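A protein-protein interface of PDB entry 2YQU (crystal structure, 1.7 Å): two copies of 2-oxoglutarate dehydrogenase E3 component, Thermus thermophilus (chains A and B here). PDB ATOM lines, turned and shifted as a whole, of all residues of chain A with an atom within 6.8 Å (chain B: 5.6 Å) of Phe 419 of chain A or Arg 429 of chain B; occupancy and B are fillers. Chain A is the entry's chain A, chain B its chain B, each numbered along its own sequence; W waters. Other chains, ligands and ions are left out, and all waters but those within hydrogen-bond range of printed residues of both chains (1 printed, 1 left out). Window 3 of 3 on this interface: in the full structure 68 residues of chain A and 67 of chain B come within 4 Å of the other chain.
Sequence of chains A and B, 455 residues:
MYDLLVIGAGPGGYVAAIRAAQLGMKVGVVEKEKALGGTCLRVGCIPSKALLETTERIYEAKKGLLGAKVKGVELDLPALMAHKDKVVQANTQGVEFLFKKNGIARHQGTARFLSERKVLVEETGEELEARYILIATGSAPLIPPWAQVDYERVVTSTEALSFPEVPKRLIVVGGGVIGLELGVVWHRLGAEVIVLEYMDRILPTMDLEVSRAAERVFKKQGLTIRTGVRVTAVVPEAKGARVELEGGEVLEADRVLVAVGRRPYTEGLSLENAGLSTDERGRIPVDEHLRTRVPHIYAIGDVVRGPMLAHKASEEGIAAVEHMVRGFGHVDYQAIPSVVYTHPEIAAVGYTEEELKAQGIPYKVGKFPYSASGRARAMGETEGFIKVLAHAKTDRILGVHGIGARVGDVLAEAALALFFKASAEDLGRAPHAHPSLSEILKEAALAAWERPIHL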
ATOM      1  N   GLU A 315     -12.381  28.115  -2.773  1.00  0.00           N
ATOM      2  CA  GLU A 315     -13.581  27.671  -3.469  1.00  0.00           C
ATOM      3  C   GLU A 315     -13.570  28.102  -4.927  1.00  0.00           C
ATOM      4  O   GLU A 315     -14.054  27.376  -5.791  1.00  0.00           O
ATOM      5  CB  GLU A 315     -14.844  28.172  -2.767  1.00  0.00           C
ATOM      6  CG  GLU A 315     -15.099  27.493  -1.427  1.00  0.00           C
ATOM      7  CD  GLU A 315     -15.626  26.075  -1.551  1.00  0.00           C
ATOM      8  OE1 GLU A 315     -15.251  25.365  -2.504  1.00  0.00           O
ATOM      9  OE2 GLU A 315     -16.416  25.657  -0.678  1.00  0.00           O
ATOM     10  N   GLU A 322     -12.315  22.908 -12.061  1.00  0.00           N
ATOM     11  CA  GLU A 322     -13.432  22.062 -12.462  1.00  0.00           C
ATOM     12  C   GLU A 322     -14.062  22.555 -13.772  1.00  0.00           C
ATOM     13  O   GLU A 322     -14.527  21.752 -14.571  1.00  0.00           O
ATOM     14  CB  GLU A 322     -14.460  21.981 -11.332  1.00  0.00           C
ATOM     15  CG  GLU A 322     -13.996  21.063 -10.213  1.00  0.00           C
ATOM     16  CD  GLU A 322     -15.023  20.855  -9.114  1.00  0.00           C
ATOM     17  OE1 GLU A 322     -14.764  19.996  -8.243  1.00  0.00           O
ATOM     18  OE2 GLU A 322     -16.076  21.543  -9.111  1.00  0.00           O
ATOM     19  N   HIS A 330     -18.985  26.475 -10.281  1.00  0.00           N
ATOM     20  CA  HIS A 330     -19.843  27.436  -9.597  1.00  0.00           C
ATOM     21  C   HIS A 330     -19.430  27.588  -8.139  1.00  0.00           C
ATOM     22  O   HIS A 330     -19.078  26.617  -7.473  1.00  0.00           O
ATOM     23  CB  HIS A 330     -21.311  26.991  -9.721  1.00  0.00           C
ATOM     24  CG  HIS A 330     -22.251  27.668  -8.772  1.00  0.00           C
ATOM     25  ND1 HIS A 330     -22.987  28.779  -9.121  1.00  0.00           N
ATOM     26  CD2 HIS A 330     -22.595  27.374  -7.496  1.00  0.00           C
ATOM     27  CE1 HIS A 330     -23.739  29.145  -8.098  1.00  0.00           C
ATOM     28  NE2 HIS A 330     -23.519  28.309  -7.099  1.00  0.00           N
ATOM     29  N   VAL A 331     -19.436  28.830  -7.669  1.00  0.00           N
ATOM     30  CA  VAL A 331     -19.238  29.135  -6.268  1.00  0.00           C
ATOM     31  C   VAL A 331     -20.523  29.740  -5.734  1.00  0.00           C
ATOM     32  O   VAL A 331     -21.107  30.626  -6.354  1.00  0.00           O
ATOM     33  CB  VAL A 331     -18.105  30.152  -6.061  1.00  0.00           C
ATOM     34  CG1 VAL A 331     -17.967  30.500  -4.574  1.00  0.00           C
ATOM     35  CG2 VAL A 331     -16.795  29.597  -6.622  1.00  0.00           C
ATOM     36  N   ASP A 332     -20.964  29.254  -4.583  1.00  0.00           N
ATOM     37  CA  ASP A 332     -22.113  29.836  -3.926  1.00  0.00           C
ATOM     38  C   ASP A 332     -21.621  30.922  -2.994  1.00  0.00           C
ATOM     39  O   ASP A 332     -21.300  30.646  -1.844  1.00  0.00           O
ATOM     40  CB  ASP A 332     -22.890  28.783  -3.147  1.00  0.00           C
ATOM     41  CG  ASP A 332     -24.179  29.325  -2.591  1.00  0.00           C
ATOM     42  OD1 ASP A 332     -24.417  30.552  -2.716  1.00  0.00           O
ATOM     43  OD2 ASP A 332     -25.019  28.600  -2.024  1.00  0.00           O
ATOM     44  N   GLN A 334     -23.213  33.245  -1.557  1.00  0.00           N
ATOM     45  CA  GLN A 334     -24.152  33.472  -0.443  1.00  0.00           C
ATOM     46  C   GLN A 334     -23.971  32.523   0.748  1.00  0.00           C
ATOM     47  O   GLN A 334     -24.549  32.747   1.822  1.00  0.00           O
ATOM     48  CB  GLN A 334     -25.591  33.357  -0.949  1.00  0.00           C
ATOM     49  CG  GLN A 334     -25.934  34.367  -2.011  1.00  0.00           C
ATOM     50  CD  GLN A 334     -25.566  35.765  -1.594  1.00  0.00           C
ATOM     51  OE1 GLN A 334     -26.141  36.301  -0.641  1.00  0.00           O
ATOM     52  NE2 GLN A 334     -24.587  36.355  -2.276  1.00  0.00           N
ATOM     53  N   ALA A 335     -23.189  31.466   0.563  1.00  0.00           N
ATOM     54  CA  ALA A 335     -22.940  30.496   1.624  1.00  0.00           C
ATOM     55  C   ALA A 335     -21.542  30.628   2.228  1.00  0.00           C
ATOM     56  O   ALA A 335     -21.136  29.787   3.019  1.00  0.00           O
ATOM     57  CB  ALA A 335     -23.159  29.087   1.098  1.00  0.00           C
ATOM     58  N   ARG A 396     -37.259  31.394   2.730  1.00  0.00           N
ATOM     59  CA  ARG A 396     -35.894  31.035   2.377  1.00  0.00           C
ATOM     60  C   ARG A 396     -34.918  31.850   3.237  1.00  0.00           C
ATOM     61  O   ARG A 396     -35.064  33.062   3.372  1.00  0.00           O
ATOM     62  CB  ARG A 396     -35.679  31.280   0.874  1.00  0.00           C
ATOM     63  CG  ARG A 396     -34.245  31.173   0.383  1.00  0.00           C
ATOM     64  CD  ARG A 396     -33.801  29.775  -0.006  1.00  0.00           C
ATOM     65  NE  ARG A 396     -32.535  29.841  -0.731  1.00  0.00           N
ATOM     66  CZ  ARG A 396     -32.411  29.892  -2.056  1.00  0.00           C
ATOM     67  NH1 ARG A 396     -33.479  29.877  -2.853  1.00  0.00           N
ATOM     68  NH2 ARG A 396     -31.197  29.953  -2.594  1.00  0.00           N
ATOM     69  N   ALA A 414     -25.092  27.542   9.752  1.00  0.00           N
ATOM     70  CA  ALA A 414     -25.868  28.528   9.005  1.00  0.00           C
ATOM     71  C   ALA A 414     -25.419  28.600   7.555  1.00  0.00           C
ATOM     72  O   ALA A 414     -26.244  28.699   6.640  1.00  0.00           O
ATOM     73  CB  ALA A 414     -25.743  29.900   9.651  1.00  0.00           C
ATOM     74  N   ALA A 415     -24.109  28.539   7.359  1.00  0.00           N
ATOM     75  CA  ALA A 415     -23.532  28.534   6.028  1.00  0.00           C
ATOM     76  C   ALA A 415     -23.998  27.294   5.261  1.00  0.00           C
ATOM     77  O   ALA A 415     -24.377  27.402   4.087  1.00  0.00           O
ATOM     78  CB  ALA A 415     -22.019  28.608   6.104  1.00  0.00           C
ATOM     79  N   LEU A 416     -24.000  26.140   5.931  1.00  0.00           N
ATOM     80  CA  LEU A 416     -24.507  24.905   5.338  1.00  0.00           C
ATOM     81  C   LEU A 416     -25.964  25.049   4.973  1.00  0.00           C
ATOM     82  O   LEU A 416     -26.359  24.665   3.881  1.00  0.00           O
ATOM     83  CB  LEU A 416     -24.337  23.702   6.260  1.00  0.00           C
ATOM     84  CG  LEU A 416     -24.660  22.341   5.618  1.00  0.00           C
ATOM     85  CD1 LEU A 416     -23.704  22.042   4.472  1.00  0.00           C
ATOM     86  CD2 LEU A 416     -24.627  21.224   6.641  1.00  0.00           C
ATOM     87  N   ALA A 417     -26.762  25.604   5.884  1.00  0.00           N
ATOM     88  CA  ALA A 417     -28.179  25.795   5.608  1.00  0.00           C
ATOM     89  C   ALA A 417     -28.389  26.658   4.353  1.00  0.00           C
ATOM     90  O   ALA A 417     -29.218  26.324   3.497  1.00  0.00           O
ATOM     91  CB  ALA A 417     -28.883  26.383   6.814  1.00  0.00           C
ATOM     92  N   LEU A 418     -27.607  27.726   4.220  1.00  0.00           N
ATOM     93  CA  LEU A 418     -27.654  28.589   3.030  1.00  0.00           C
ATOM     94  C   LEU A 418     -27.251  27.843   1.758  1.00  0.00           C
ATOM     95  O   LEU A 418     -27.893  28.006   0.713  1.00  0.00           O
ATOM     96  CB  LEU A 418     -26.763  29.817   3.227  1.00  0.00           C
ATOM     97  CG  LEU A 418     -27.528  30.940   3.929  1.00  0.00           C
ATOM     98  CD1 LEU A 418     -26.619  31.836   4.737  1.00  0.00           C
ATOM     99  CD2 LEU A 418     -28.305  31.756   2.905  1.00  0.00           C
ATOM    100  N   PHE A 419     -26.208  27.022   1.860  1.00  0.00           N
ATOM    101  CA  PHE A 419     -25.748  26.173   0.754  1.00  0.00           C
ATOM    102  C   PHE A 419     -26.847  25.205   0.325  1.00  0.00           C
ATOM    103  O   PHE A 419     -27.003  24.941  -0.858  1.00  0.00           O
ATOM    104  CB  PHE A 419     -24.488  25.388   1.156  1.00  0.00           C
ATOM    105  CG  PHE A 419     -23.822  24.672   0.015  1.00  0.00           C
ATOM    106  CD1 PHE A 419     -23.245  25.388  -1.023  1.00  0.00           C
ATOM    107  CD2 PHE A 419     -23.752  23.281  -0.010  1.00  0.00           C
ATOM    108  CE1 PHE A 419     -22.613  24.734  -2.067  1.00  0.00           C
ATOM    109  CE2 PHE A 419     -23.120  22.625  -1.062  1.00  0.00           C
ATOM    110  CZ  PHE A 419     -22.560  23.356  -2.091  1.00  0.00           C
ATOM    111  N   PHE A 420     -27.628  24.723   1.295  1.00  0.00           N
ATOM    112  CA  PHE A 420     -28.744  23.806   1.036  1.00  0.00           C
ATOM    113  C   PHE A 420     -30.031  24.541   0.650  1.00  0.00           C
ATOM    114  O   PHE A 420     -31.066  23.898   0.468  1.00  0.00           O
ATOM    115  CB  PHE A 420     -29.041  22.955   2.283  1.00  0.00           C
ATOM    116  CG  PHE A 420     -28.034  21.861   2.559  1.00  0.00           C
ATOM    117  CD1 PHE A 420     -26.990  21.588   1.684  1.00  0.00           C
ATOM    118  CD2 PHE A 420     -28.145  21.098   3.709  1.00  0.00           C
ATOM    119  CE1 PHE A 420     -26.091  20.585   1.950  1.00  0.00           C
ATOM    120  CE2 PHE A 420     -27.236  20.097   3.979  1.00  0.00           C
ATOM    121  CZ  PHE A 420     -26.207  19.843   3.097  1.00  0.00           C
ATOM    122  N   LYS A 421     -29.974  25.872   0.544  1.00  0.00           N
ATOM    123  CA  LYS A 421     -31.134  26.701   0.184  1.00  0.00           C
ATOM    124  C   LYS A 421     -32.285  26.462   1.159  1.00  0.00           C
ATOM    125  O   LYS A 421     -33.461  26.419   0.776  1.00  0.00           O
ATOM    126  CB  LYS A 421     -31.561  26.448  -1.269  1.00  0.00           C
ATOM    127  CG  LYS A 421     -30.408  26.620  -2.265  1.00  0.00           C
ATOM    128  CD  LYS A 421     -30.891  26.689  -3.711  1.00  0.00           C
ATOM    129  CE  LYS A 421     -29.841  27.308  -4.632  1.00  0.00           C
ATOM    130  NZ  LYS A 421     -28.581  26.524  -4.680  1.00  0.00           N
ATOM    131  N   ALA A 422     -31.913  26.341   2.428  1.00  0.00           N
ATOM    132  CA  ALA A 422     -32.833  25.979   3.504  1.00  0.00           C
ATOM    133  C   ALA A 422     -33.794  27.098   3.797  1.00  0.00           C
ATOM    134  O   ALA A 422     -33.471  28.269   3.616  1.00  0.00           O
ATOM    135  CB  ALA A 422     -32.057  25.660   4.771  1.00  0.00           C
ATOM    136  N   ALA B 424     -22.573  12.960   1.436  1.00  0.00           N
ATOM    137  CA  ALA B 424     -21.251  13.374   1.898  1.00  0.00           C
ATOM    138  C   ALA B 424     -20.705  14.460   0.976  1.00  0.00           C
ATOM    139  O   ALA B 424     -20.136  15.451   1.440  1.00  0.00           O
ATOM    140  CB  ALA B 424     -20.306  12.183   1.940  1.00  0.00           C
ATOM    141  N   GLU B 425     -20.900  14.271  -0.329  1.00  0.00           N
ATOM    142  CA  GLU B 425     -20.528  15.266  -1.336  1.00  0.00           C
ATOM    143  C   GLU B 425     -21.165  16.633  -1.079  1.00  0.00           C
ATOM    144  O   GLU B 425     -20.494  17.648  -1.200  1.00  0.00           O
ATOM    145  CB  GLU B 425     -20.915  14.809  -2.748  1.00  0.00           C
ATOM    146  CG  GLU B 425     -20.135  15.534  -3.832  1.00  0.00           C
ATOM    147  CD  GLU B 425     -20.629  15.279  -5.248  1.00  0.00           C
ATOM    148  OE1 GLU B 425     -21.618  14.531  -5.454  1.00  0.00           O
ATOM    149  OE2 GLU B 425     -20.011  15.854  -6.175  1.00  0.00           O
ATOM    150  N   ASP B 426     -22.454  16.657  -0.738  1.00  0.00           N
ATOM    151  CA  ASP B 426     -23.163  17.909  -0.469  1.00  0.00           C
ATOM    152  C   ASP B 426     -22.472  18.670   0.658  1.00  0.00           C
ATOM    153  O   ASP B 426     -22.223  19.873   0.557  1.00  0.00           O
ATOM    154  CB  ASP B 426     -24.613  17.650  -0.041  1.00  0.00           C
ATOM    155  CG  ASP B 426     -25.491  17.151  -1.167  1.00  0.00           C
ATOM    156  OD1 ASP B 426     -26.528  16.522  -0.860  1.00  0.00           O
ATOM    157  OD2 ASP B 426     -25.228  17.332  -2.377  1.00  0.00           O
ATOM    158  N   LEU B 427     -22.176  17.946   1.732  1.00  0.00           N
ATOM    159  CA  LEU B 427     -21.547  18.516   2.919  1.00  0.00           C
ATOM    160  C   LEU B 427     -20.112  18.950   2.640  1.00  0.00           C
ATOM    161  O   LEU B 427     -19.696  20.039   3.026  1.00  0.00           O
ATOM    162  CB  LEU B 427     -21.575  17.491   4.057  1.00  0.00           C
ATOM    163  CG  LEU B 427     -20.932  17.874   5.386  1.00  0.00           C
ATOM    164  CD1 LEU B 427     -21.502  19.183   5.898  1.00  0.00           C
ATOM    165  CD2 LEU B 427     -21.142  16.764   6.398  1.00  0.00           C
ATOM    166  N   GLY B 428     -19.370  18.098   1.949  1.00  0.00           N
ATOM    167  CA  GLY B 428     -17.975  18.348   1.653  1.00  0.00           C
ATOM    168  C   GLY B 428     -17.757  19.501   0.693  1.00  0.00           C
ATOM    169  O   GLY B 428     -16.697  20.125   0.712  1.00  0.00           O
ATOM    170  N   ARG B 429     -18.751  19.782  -0.154  1.00  0.00           N
ATOM    171  CA  ARG B 429     -18.638  20.845  -1.150  1.00  0.00           C
ATOM    172  C   ARG B 429     -18.991  22.207  -0.563  1.00  0.00           C
ATOM    173  O   ARG B 429     -18.580  23.224  -1.090  1.00  0.00           O
ATOM    174  CB  ARG B 429     -19.566  20.588  -2.342  1.00  0.00           C
ATOM    175  CG  ARG B 429     -19.028  19.617  -3.389  1.00  0.00           C
ATOM    176  CD  ARG B 429     -20.062  19.283  -4.471  1.00  0.00           C
ATOM    177  NE  ARG B 429     -20.722  20.497  -4.968  1.00  0.00           N
ATOM    178  CZ  ARG B 429     -22.001  20.605  -5.323  1.00  0.00           C
ATOM    179  NH1 ARG B 429     -22.828  19.561  -5.268  1.00  0.00           N
ATOM    180  NH2 ARG B 429     -22.459  21.777  -5.745  1.00  0.00           N
ATOM    181  N   ALA B 430     -19.781  22.225   0.509  1.00  0.00           N
ATOM    182  CA  ALA B 430     -20.247  23.475   1.109  1.00  0.00           C
ATOM    183  C   ALA B 430     -19.053  24.327   1.550  1.00  0.00           C
ATOM    184  O   ALA B 430     -18.065  23.785   2.029  1.00  0.00           O
ATOM    185  CB  ALA B 430     -21.122  23.175   2.289  1.00  0.00           C
ATOM    186  N   PRO B 431     -19.112  25.643   1.351  1.00  0.00           N
ATOM    187  CA  PRO B 431     -18.103  26.531   1.939  1.00  0.00           C
ATOM    188  C   PRO B 431     -17.990  26.377   3.458  1.00  0.00           C
ATOM    189  O   PRO B 431     -18.991  26.230   4.154  1.00  0.00           O
ATOM    190  CB  PRO B 431     -18.592  27.929   1.548  1.00  0.00           C
ATOM    191  CG  PRO B 431     -19.407  27.732   0.333  1.00  0.00           C
ATOM    192  CD  PRO B 431     -20.061  26.384   0.494  1.00  0.00           C
ATOM    193  N   LYS B 442     -15.782  19.107   6.968  1.00  0.00           N
ATOM    194  CA  LYS B 442     -15.760  19.267   5.515  1.00  0.00           C
ATOM    195  C   LYS B 442     -14.857  18.223   4.874  1.00  0.00           C
ATOM    196  O   LYS B 442     -15.272  17.534   3.941  1.00  0.00           O
ATOM    197  CB  LYS B 442     -15.271  20.672   5.126  1.00  0.00           C
ATOM    198  CG  LYS B 442     -14.983  20.857   3.630  1.00  0.00           C
ATOM    199  CD  LYS B 442     -14.475  22.266   3.285  1.00  0.00           C
ATOM    200  CE  LYS B 442     -14.218  22.426   1.785  1.00  0.00           C
ATOM    201  NZ  LYS B 442     -15.479  22.706   1.001  1.00  0.00           N
ATOM    202  N   LEU B 446     -15.738  14.958   2.422  1.00  0.00           N
ATOM    203  CA  LEU B 446     -15.129  14.773   1.105  1.00  0.00           C
ATOM    204  C   LEU B 446     -14.433  13.417   1.026  1.00  0.00           C
ATOM    205  O   LEU B 446     -14.472  12.753  -0.021  1.00  0.00           O
ATOM    206  CB  LEU B 446     -14.115  15.883   0.809  1.00  0.00           C
ATOM    207  CG  LEU B 446     -14.633  17.291   0.501  1.00  0.00           C
ATOM    208  CD1 LEU B 446     -13.469  18.264   0.447  1.00  0.00           C
ATOM    209  CD2 LEU B 446     -15.427  17.329  -0.800  1.00  0.00           C
HETATM  210  O   HOH W   1     -14.528  25.587   2.080  1.00  0.00           O
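Arg 396 of chain A touches none of the printed residues of chain B.
Of the printed residues of chain B, Leu 416 of chain A touches Leu 427 (3.8 Å) and Ala 430 (3.6 Å).
Of the printed residues of chain B, Phe 419 of chain A touches Asp 426 (3.3 Å), Arg 429 (3.98 Å), Ala 430 (3.5 Å) and Pro 431 (3.7 Å).
Of the printed residues of chain A, Arg 429 of chain B touches Glu 315 and Phe 419.
Of the printed residues of chain A, Lys 442 of chain B touches Glu 315 (3.5 Å).
Glu 315 of chain A touches Ala 430 of chain B.
Ala 335 of chain A touches Pro 431 of chain B (O to CB, 3.5 Å).
Leu 427 of chain B touches Leu 416 of chain A.
CB of Ala 430 of chain B touches CD1 of Leu 416 of chain A, 3.6 Å away.
CE2 of Phe 419 of chain A touches O of Asp 426 of chain B (3.3 Å).
Phe 419 of chain A touches Arg 429 of chain B.
CB of Ala 430 of chain B touches CD2 of Phe 419 of chain A, 3.5 Å away.
CD1 of Phe 419 of chain A touches CD of Pro 431 of chain B, 3.7 Å away.
Phe 420 of chain A touches Asp 426 of chain B (CE1 to CB, 3.8 Å).
Hydrophobic or aromatic side chains of chain B within 4 Å of the printed part of chain A: Leu 427, Ala 430 and Pro 431.
Hydrophobic or aromatic side chains of chain A within 4 Å of the printed part of chain B: Leu 416, Phe 419 and Phe 420.
Among the printed residues, 12 pairs touch across the chains.
Among the printed residues, Asp or Glu carboxylates within 4 Å of a Lys or Arg side-chain nitrogen of the other chain: Glu 315 of chain A with Lys 442 of chain B.
Water W1 bridges the side-chain amino group (NZ) of Lys 442 of chain B and the side-chain carboxylate (OE2) of Glu 315 of chain A.
The side-chain carboxylate of Glu 315 of chain A sits close to the backbone carbonyl oxygen of Arg 429 of chain B, at 3.3 Å.
NZ of Lys 442 of chain B lies within salt-bridge range of OE2 of Glu 315 of chain A (3.5 Å).
The side-chain carboxylate (OE2) of Glu 315 of chain A sits close to the backbone nitrogen (N) of Pro 431 of chain B (3.4 Å).
No position is printed for both chains.
Of the 12 pairs that touch across the chains among the printed residues, none has its exchanged pair printed and touching as well.
The backbone carbonyl oxygen (O) of Gly 428 of chain B sits at hydrogen-bond distance from the side-chain amino group (NZ) of Lys 442 of chain B, at 2.9 Å.
The backbone carbonyl oxygen (O) of Ala 430 of chain B is in hydrogen-bond range of the side-chain amino group (NZ) of Lys 442 of chain B (3.0 Å).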
